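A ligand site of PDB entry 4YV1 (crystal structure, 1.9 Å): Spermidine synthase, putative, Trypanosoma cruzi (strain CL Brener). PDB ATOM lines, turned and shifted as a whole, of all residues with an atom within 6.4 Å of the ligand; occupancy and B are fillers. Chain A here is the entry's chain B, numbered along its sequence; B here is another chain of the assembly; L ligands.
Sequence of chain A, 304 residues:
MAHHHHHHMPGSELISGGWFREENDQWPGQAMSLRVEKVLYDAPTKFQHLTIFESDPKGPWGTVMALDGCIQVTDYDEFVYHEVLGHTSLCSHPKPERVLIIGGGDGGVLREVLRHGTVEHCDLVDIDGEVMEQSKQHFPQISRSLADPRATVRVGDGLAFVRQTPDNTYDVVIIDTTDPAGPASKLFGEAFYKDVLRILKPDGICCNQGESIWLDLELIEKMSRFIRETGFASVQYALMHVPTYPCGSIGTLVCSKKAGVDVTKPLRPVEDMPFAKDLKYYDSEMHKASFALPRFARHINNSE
An oxygen (O1) of the ligand lies close to the side-chain amide oxygen of Gln 30, at 3.2 Å. The backbone NH of Cys 247 sits at hydrogen-bond distance from an oxygen (O1) of the ligand, at 2.8 Å.
The side-chain amide nitrogen of Gln 30 sits close to the indole nitrogen of Trp 61 of chain B (3.1 Å). The side-chain hydroxyl of Thr 244 of chain B is in hydrogen-bond range of the side-chain carboxylate of Asp 77 of chain B, 2.6 Å away. N of Glu 22 lies within hydrogen-bond range of O of Met 32 of chain A (2.8 Å). O of Ala 31 sits at hydrogen-bond distance from N of Ser 33 of chain B (2.8 Å).
Merely in contact with the ligand: Glu 22 (3.2 Å), Met 32 of chain A (3.3 Å), Pro 246 (3.5 Å), Pro 243 of chain B (3.5 Å), Trp 27 (3.5 Å), Trp 61 of chain B (3.6 Å), Thr 244 of chain B (3.6 Å), Met 32 of chain B (3.8 Å), Tyr 245 of chain A (3.8 Å), Leu 34 of chain B (3.8 Å) and Ala 31 (3.9 Å). Hydrophobic or aromatic side chains that line the ligand: Trp 27, Met 32 of chain A, Pro 246, Met 32 of chain B, Leu 34 of chain B and Trp 61 of chain B. 13 residues have an atom within 4 Å of the ligand: Glu 22, Trp 27, Gln 30, Ala 31, Met 32 of chain A, Tyr 245 of chain A, Pro 246, Cys 247, Met 32 of chain B, Leu 34 of chain B, Trp 61 of chain B, Pro 243 of chain B and Thr 244 of chain B.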
ATOM      1  N   GLU A  22     -13.367   5.129  15.260  1.00  0.00           N
ATOM      2  CA  GLU A  22     -13.876   6.264  15.997  1.00  0.00           C
ATOM      3  C   GLU A  22     -14.104   5.799  17.448  1.00  0.00           C
ATOM      4  O   GLU A  22     -14.956   4.944  17.727  1.00  0.00           O
ATOM      5  CB  GLU A  22     -15.191   6.666  15.302  1.00  0.00           C
ATOM      6  CG  GLU A  22     -15.884   7.921  15.780  1.00  0.00           C
ATOM      7  CD  GLU A  22     -16.940   8.347  14.759  1.00  0.00           C
ATOM      8  OE1 GLU A  22     -17.856   7.553  14.434  1.00  0.00           O
ATOM      9  OE2 GLU A  22     -16.832   9.458  14.232  1.00  0.00           O
ATOM     10  N   GLU A  23     -13.313   6.339  18.373  1.00  0.00           N
ATOM     11  CA  GLU A  23     -13.439   6.058  19.817  1.00  0.00           C
ATOM     12  C   GLU A  23     -13.383   7.430  20.473  1.00  0.00           C
ATOM     13  O   GLU A  23     -12.625   8.303  20.042  1.00  0.00           O
ATOM     14  CB  GLU A  23     -12.255   5.220  20.258  1.00  0.00           C
ATOM     15  CG  GLU A  23     -12.471   4.229  21.382  1.00  0.00           C
ATOM     16  CD  GLU A  23     -11.266   3.292  21.537  1.00  0.00           C
ATOM     17  OE1 GLU A  23     -10.703   3.257  22.646  1.00  0.00           O
ATOM     18  OE2 GLU A  23     -10.880   2.577  20.569  1.00  0.00           O
ATOM     19  N   ASN A  24     -14.184   7.642  21.497  1.00  0.00           N
ATOM     20  CA  ASN A  24     -14.179   8.909  22.235  1.00  0.00           C
ATOM     21  C   ASN A  24     -14.058   8.608  23.705  1.00  0.00           C
ATOM     22  O   ASN A  24     -14.930   7.937  24.247  1.00  0.00           O
ATOM     23  CB  ASN A  24     -15.478   9.669  21.990  1.00  0.00           C
ATOM     24  CG  ASN A  24     -15.285  11.179  21.991  1.00  0.00           C
ATOM     25  OD1 ASN A  24     -15.312  11.817  23.040  1.00  0.00           O
ATOM     26  ND2 ASN A  24     -15.089  11.751  20.802  1.00  0.00           N
ATOM     27  N   TRP A  27     -16.601   8.748  26.095  1.00  0.00           N
ATOM     28  CA  TRP A  27     -17.490   7.556  26.115  1.00  0.00           C
ATOM     29  C   TRP A  27     -16.688   6.227  26.144  1.00  0.00           C
ATOM     30  O   TRP A  27     -16.651   5.498  25.144  1.00  0.00           O
ATOM     31  CB  TRP A  27     -18.475   7.618  24.931  1.00  0.00           C
ATOM     32  CG  TRP A  27     -18.985   9.044  24.574  1.00  0.00           C
ATOM     33  CD1 TRP A  27     -19.579   9.953  25.421  1.00  0.00           C
ATOM     34  CD2 TRP A  27     -18.936   9.674  23.268  1.00  0.00           C
ATOM     35  NE1 TRP A  27     -19.897  11.108  24.729  1.00  0.00           N
ATOM     36  CE2 TRP A  27     -19.519  10.969  23.419  1.00  0.00           C
ATOM     37  CE3 TRP A  27     -18.470   9.273  22.002  1.00  0.00           C
ATOM     38  CZ2 TRP A  27     -19.636  11.867  22.338  1.00  0.00           C
ATOM     39  CZ3 TRP A  27     -18.577  10.178  20.926  1.00  0.00           C
ATOM     40  CH2 TRP A  27     -19.159  11.459  21.097  1.00  0.00           C
ATOM     41  N   GLN A  30     -16.137   1.827  23.920  1.00  0.00           N
ATOM     42  CA  GLN A  30     -16.951   1.514  22.711  1.00  0.00           C
ATOM     43  C   GLN A  30     -16.222   2.140  21.514  1.00  0.00           C
ATOM     44  O   GLN A  30     -15.606   3.180  21.685  1.00  0.00           O
ATOM     45  CB  GLN A  30     -18.407   2.085  22.827  1.00  0.00           C
ATOM     46  CG  GLN A  30     -18.533   3.600  23.094  1.00  0.00           C
ATOM     47  CD  GLN A  30     -19.994   4.095  23.230  1.00  0.00           C
ATOM     48  OE1 GLN A  30     -20.644   4.473  22.229  1.00  0.00           O
ATOM     49  NE2 GLN A  30     -20.487   4.166  24.476  1.00  0.00           N
ATOM     50  N   ALA A  31     -16.284   1.502  20.345  1.00  0.00           N
ATOM     51  CA  ALA A  31     -15.758   2.056  19.082  1.00  0.00           C
ATOM     52  C   ALA A  31     -16.638   1.604  17.918  1.00  0.00           C
ATOM     53  O   ALA A  31     -17.362   0.593  18.045  1.00  0.00           O
ATOM     54  CB  ALA A  31     -14.279   1.679  18.876  1.00  0.00           C
ATOM     55  N   MET A  32     -16.638   2.384  16.830  1.00  0.00           N
ATOM     56  CA  MET A  32     -17.243   2.063  15.556  1.00  0.00           C
ATOM     57  C   MET A  32     -16.151   2.242  14.506  1.00  0.00           C
ATOM     58  O   MET A  32     -15.294   3.127  14.676  1.00  0.00           O
ATOM     59  CB  MET A  32     -18.369   3.015  15.177  1.00  0.00           C
ATOM     60  CG  MET A  32     -19.128   2.533  13.934  1.00  0.00           C
ATOM     61  SD  MET A  32     -19.498   3.740  12.607  1.00  0.00           S
ATOM     62  CE  MET A  32     -20.710   2.840  11.614  1.00  0.00           C
ATOM     63  N   ILE A  71     -17.197  11.285  12.780  1.00  0.00           N
ATOM     64  CA  ILE A  71     -17.963  11.342  11.528  1.00  0.00           C
ATOM     65  C   ILE A  71     -19.016  12.488  11.550  1.00  0.00           C
ATOM     66  O   ILE A  71     -19.791  12.562  12.483  1.00  0.00           O
ATOM     67  CB  ILE A  71     -18.631   9.960  11.233  1.00  0.00           C
ATOM     68  CG1 ILE A  71     -17.556   8.923  10.935  1.00  0.00           C
ATOM     69  CG2 ILE A  71     -19.550  10.059  10.014  1.00  0.00           C
ATOM     70  CD1 ILE A  71     -18.137   7.528  10.837  1.00  0.00           C
ATOM     71  N   LEU A 215     -25.905   9.666  25.576  1.00  0.00           N
ATOM     72  CA  LEU A 215     -24.579   9.991  26.037  1.00  0.00           C
ATOM     73  C   LEU A 215     -24.505  11.305  26.757  1.00  0.00           C
ATOM     74  O   LEU A 215     -23.574  11.459  27.482  1.00  0.00           O
ATOM     75  CB  LEU A 215     -23.589  10.005  24.857  1.00  0.00           C
ATOM     76  CG  LEU A 215     -23.582   8.633  24.164  1.00  0.00           C
ATOM     77  CD1 LEU A 215     -22.921   8.762  22.805  1.00  0.00           C
ATOM     78  CD2 LEU A 215     -22.888   7.596  25.034  1.00  0.00           C
ATOM     79  N   PRO A 243     -27.731   6.745  11.879  1.00  0.00           N
ATOM     80  CA  PRO A 243     -26.956   5.555  12.233  1.00  0.00           C
ATOM     81  C   PRO A 243     -25.451   5.789  12.427  1.00  0.00           C
ATOM     82  O   PRO A 243     -24.772   4.974  13.095  1.00  0.00           O
ATOM     83  CB  PRO A 243     -27.136   4.624  11.032  1.00  0.00           C
ATOM     84  CG  PRO A 243     -28.161   5.215  10.157  1.00  0.00           C
ATOM     85  CD  PRO A 243     -28.387   6.663  10.553  1.00  0.00           C
ATOM     86  N   THR A 244     -24.878   6.784  11.793  1.00  0.00           N
ATOM     87  CA  THR A 244     -23.426   6.965  11.923  1.00  0.00           C
ATOM     88  C   THR A 244     -23.038   7.886  13.084  1.00  0.00           C
ATOM     89  O   THR A 244     -21.879   8.292  13.211  1.00  0.00           O
ATOM     90  CB  THR A 244     -22.828   7.571  10.627  1.00  0.00           C
ATOM     91  OG1 THR A 244     -23.520   8.776  10.327  1.00  0.00           O
ATOM     92  CG2 THR A 244     -23.052   6.614   9.437  1.00  0.00           C
ATOM     93  N   TYR A 245     -24.034   8.297  13.877  1.00  0.00           N
ATOM     94  CA  TYR A 245     -23.733   9.160  14.997  1.00  0.00           C
ATOM     95  C   TYR A 245     -23.669   8.240  16.184  1.00  0.00           C
ATOM     96  O   TYR A 245     -24.287   7.196  16.214  1.00  0.00           O
ATOM     97  CB  TYR A 245     -24.739  10.336  15.167  1.00  0.00           C
ATOM     98  CG  TYR A 245     -24.588  11.534  14.198  1.00  0.00           C
ATOM     99  CD1 TYR A 245     -23.450  11.712  13.360  1.00  0.00           C
ATOM    100  CD2 TYR A 245     -25.590  12.512  14.116  1.00  0.00           C
ATOM    101  CE1 TYR A 245     -23.340  12.817  12.510  1.00  0.00           C
ATOM    102  CE2 TYR A 245     -25.478  13.619  13.241  1.00  0.00           C
ATOM    103  CZ  TYR A 245     -24.381  13.761  12.444  1.00  0.00           C
ATOM    104  OH  TYR A 245     -24.322  14.876  11.611  1.00  0.00           O
ATOM    105  N   PRO A 246     -22.882   8.594  17.202  1.00  0.00           N
ATOM    106  CA  PRO A 246     -22.726   7.754  18.371  1.00  0.00           C
ATOM    107  C   PRO A 246     -24.045   7.305  19.026  1.00  0.00           C
ATOM    108  O   PRO A 246     -24.915   8.146  19.318  1.00  0.00           O
ATOM    109  CB  PRO A 246     -22.007   8.684  19.362  1.00  0.00           C
ATOM    110  CG  PRO A 246     -21.250   9.634  18.480  1.00  0.00           C
ATOM    111  CD  PRO A 246     -22.117   9.863  17.260  1.00  0.00           C
ATOM    112  N   CYS A 247     -24.197   5.988  19.223  1.00  0.00           N
ATOM    113  CA  CYS A 247     -25.393   5.339  19.765  1.00  0.00           C
ATOM    114  C   CYS A 247     -26.627   5.474  18.851  1.00  0.00           C
ATOM    115  O   CYS A 247     -27.721   5.139  19.278  1.00  0.00           O
ATOM    116  CB  CYS A 247     -25.784   5.879  21.158  1.00  0.00           C
ATOM    117  SG  CYS A 247     -24.631   5.260  22.416  1.00  0.00           S
ATOM    118  N   GLY A 248     -26.442   5.988  17.650  1.00  0.00           N
ATOM    119  CA  GLY A 248     -27.464   5.894  16.574  1.00  0.00           C
ATOM    120  C   GLY A 248     -28.563   6.937  16.547  1.00  0.00           C
ATOM    121  O   GLY A 248     -29.540   6.815  15.779  1.00  0.00           O
ATOM    122  N   MET B  32     -18.549  -2.697  15.034  1.00  0.00           N
ATOM    123  CA  MET B  32     -18.848  -2.052  16.336  1.00  0.00           C
ATOM    124  C   MET B  32     -18.092  -2.853  17.399  1.00  0.00           C
ATOM    125  O   MET B  32     -18.098  -4.097  17.360  1.00  0.00           O
ATOM    126  CB  MET B  32     -20.377  -2.144  16.629  1.00  0.00           C
ATOM    127  CG  MET B  32     -21.227  -0.935  16.233  1.00  0.00           C
ATOM    128  SD  MET B  32     -23.028  -1.129  15.896  1.00  0.00           S
ATOM    129  CE  MET B  32     -23.530  -2.491  16.952  1.00  0.00           C
ATOM    130  N   SER B  33     -17.434  -2.192  18.355  1.00  0.00           N
ATOM    131  CA  SER B  33     -16.625  -2.953  19.326  1.00  0.00           C
ATOM    132  C   SER B  33     -16.885  -2.482  20.752  1.00  0.00           C
ATOM    133  O   SER B  33     -17.164  -1.314  20.978  1.00  0.00           O
ATOM    134  CB  SER B  33     -15.155  -2.859  18.964  1.00  0.00           C
ATOM    135  OG  SER B  33     -14.959  -3.392  17.645  1.00  0.00           O
ATOM    136  N   LEU B  34     -16.825  -3.413  21.713  1.00  0.00           N
ATOM    137  CA  LEU B  34     -16.937  -3.061  23.126  1.00  0.00           C
ATOM    138  C   LEU B  34     -15.773  -3.666  23.862  1.00  0.00           C
ATOM    139  O   LEU B  34     -15.360  -4.786  23.557  1.00  0.00           O
ATOM    140  CB  LEU B  34     -18.227  -3.584  23.746  1.00  0.00           C
ATOM    141  CG  LEU B  34     -19.547  -2.953  23.322  1.00  0.00           C
ATOM    142  CD1 LEU B  34     -20.709  -3.800  23.838  1.00  0.00           C
ATOM    143  CD2 LEU B  34     -19.576  -1.524  23.848  1.00  0.00           C
ATOM    144  N   TRP B  61     -22.534   0.213  29.588  1.00  0.00           N
ATOM    145  CA  TRP B  61     -23.268  -0.964  29.029  1.00  0.00           C
ATOM    146  C   TRP B  61     -23.466  -2.093  30.040  1.00  0.00           C
ATOM    147  O   TRP B  61     -24.403  -2.877  29.936  1.00  0.00           O
ATOM    148  CB  TRP B  61     -22.578  -1.439  27.721  1.00  0.00           C
ATOM    149  CG  TRP B  61     -22.455  -0.262  26.781  1.00  0.00           C
ATOM    150  CD1 TRP B  61     -21.324   0.449  26.464  1.00  0.00           C
ATOM    151  CD2 TRP B  61     -23.551   0.409  26.098  1.00  0.00           C
ATOM    152  NE1 TRP B  61     -21.645   1.499  25.599  1.00  0.00           N
ATOM    153  CE2 TRP B  61     -23.001   1.480  25.369  1.00  0.00           C
ATOM    154  CE3 TRP B  61     -24.947   0.185  26.028  1.00  0.00           C
ATOM    155  CZ2 TRP B  61     -23.808   2.364  24.586  1.00  0.00           C
ATOM    156  CZ3 TRP B  61     -25.742   1.044  25.256  1.00  0.00           C
ATOM    157  CH2 TRP B  61     -25.163   2.130  24.558  1.00  0.00           C
ATOM    158  N   ILE B  71     -24.687  -8.909  19.386  1.00  0.00           N
ATOM    159  CA  ILE B  71     -25.219  -8.463  20.687  1.00  0.00           C
ATOM    160  C   ILE B  71     -26.725  -8.664  20.721  1.00  0.00           C
ATOM    161  O   ILE B  71     -27.419  -8.377  19.744  1.00  0.00           O
ATOM    162  CB  ILE B  71     -24.776  -7.040  21.056  1.00  0.00           C
ATOM    163  CG1 ILE B  71     -23.248  -7.070  21.298  1.00  0.00           C
ATOM    164  CG2 ILE B  71     -25.514  -6.571  22.319  1.00  0.00           C
ATOM    165  CD1 ILE B  71     -22.546  -5.734  21.203  1.00  0.00           C
ATOM    166  N   ASP B  77     -29.297  -1.105  27.954  1.00  0.00           N
ATOM    167  CA  ASP B  77     -30.408  -0.757  27.024  1.00  0.00           C
ATOM    168  C   ASP B  77     -31.443  -1.797  26.793  1.00  0.00           C
ATOM    169  O   ASP B  77     -32.330  -1.615  25.929  1.00  0.00           O
ATOM    170  CB  ASP B  77     -29.880  -0.240  25.653  1.00  0.00           C
ATOM    171  CG  ASP B  77     -29.163  -1.305  24.842  1.00  0.00           C
ATOM    172  OD1 ASP B  77     -28.995  -2.463  25.335  1.00  0.00           O
ATOM    173  OD2 ASP B  77     -28.719  -0.952  23.686  1.00  0.00           O
ATOM    174  N   PRO B 243     -29.327   1.459  21.029  1.00  0.00           N
ATOM    175  CA  PRO B 243     -27.952   1.927  20.747  1.00  0.00           C
ATOM    176  C   PRO B 243     -27.015   0.768  20.372  1.00  0.00           C
ATOM    177  O   PRO B 243     -26.128   0.907  19.483  1.00  0.00           O
ATOM    178  CB  PRO B 243     -27.538   2.594  22.056  1.00  0.00           C
ATOM    179  CG  PRO B 243     -28.793   2.880  22.800  1.00  0.00           C
ATOM    180  CD  PRO B 243     -29.842   1.924  22.327  1.00  0.00           C
ATOM    181  N   THR B 244     -27.274  -0.414  20.913  1.00  0.00           N
ATOM    182  CA  THR B 244     -26.284  -1.495  20.682  1.00  0.00           C
ATOM    183  C   THR B 244     -26.683  -2.390  19.509  1.00  0.00           C
ATOM    184  O   THR B 244     -26.058  -3.432  19.300  1.00  0.00           O
ATOM    185  CB  THR B 244     -26.181  -2.393  21.930  1.00  0.00           C
ATOM    186  OG1 THR B 244     -27.516  -2.748  22.315  1.00  0.00           O
ATOM    187  CG2 THR B 244     -25.503  -1.670  23.104  1.00  0.00           C
ATOM    188  N   TYR B 245     -27.747  -2.056  18.785  1.00  0.00           N
ATOM    189  CA  TYR B 245     -28.050  -2.877  17.631  1.00  0.00           C
ATOM    190  C   TYR B 245     -27.472  -2.173  16.412  1.00  0.00           C
ATOM    191  O   TYR B 245     -27.282  -0.937  16.439  1.00  0.00           O
ATOM    192  CB  TYR B 245     -29.574  -3.146  17.508  1.00  0.00           C
ATOM    193  CG  TYR B 245     -30.149  -4.179  18.524  1.00  0.00           C
ATOM    194  CD1 TYR B 245     -29.334  -5.103  19.212  1.00  0.00           C
ATOM    195  CD2 TYR B 245     -31.536  -4.256  18.765  1.00  0.00           C
ATOM    196  CE1 TYR B 245     -29.885  -6.043  20.124  1.00  0.00           C
ATOM    197  CE2 TYR B 245     -32.083  -5.189  19.662  1.00  0.00           C
ATOM    198  CZ  TYR B 245     -31.268  -6.099  20.329  1.00  0.00           C
ATOM    199  OH  TYR B 245     -31.861  -7.015  21.203  1.00  0.00           O
HETATM  200  C1  LIG L   1     -20.977   5.407  15.870  1.00  0.00           C
HETATM  201  C2  LIG L   1     -17.967   7.157  19.191  1.00  0.00           C
HETATM  202  C3  LIG L   1     -20.173   6.424  16.351  1.00  0.00           C
HETATM  203  C4  LIG L   1     -18.674   7.295  18.009  1.00  0.00           C
HETATM  204  C5  LIG L   1     -21.075   4.250  16.596  1.00  0.00           C
HETATM  205  C6  LIG L   1     -18.094   5.965  19.871  1.00  0.00           C
HETATM  206  C7  LIG L   1     -19.472   6.275  17.540  1.00  0.00           C
HETATM  207  C8  LIG L   1     -19.562   5.118  18.287  1.00  0.00           C
HETATM  208  C9  LIG L   1     -20.381   4.117  17.777  1.00  0.00           C
HETATM  209  C10 LIG L   1     -21.520   3.078  19.375  1.00  0.00           C
HETATM  210  C11 LIG L   1     -22.188  -0.622  21.235  1.00  0.00           C
HETATM  211  C12 LIG L   1     -23.181   0.511  21.379  1.00  0.00           C
HETATM  212  C13 LIG L   1     -21.390  -0.507  19.970  1.00  0.00           C
HETATM  213  C14 LIG L   1     -22.531   1.871  21.283  1.00  0.00           C
HETATM  214  C15 LIG L   1     -20.674   0.819  19.995  1.00  0.00           C
HETATM  215  N1  LIG L   1     -18.874   4.971  19.442  1.00  0.00           N
HETATM  216  N2  LIG L   1     -21.608   1.930  20.163  1.00  0.00           N
HETATM  217  O1  LIG L   1     -22.240   4.075  19.501  1.00  0.00           O
HETATM  218  O2  LIG L   1     -20.505   2.917  18.461  1.00  0.00           O
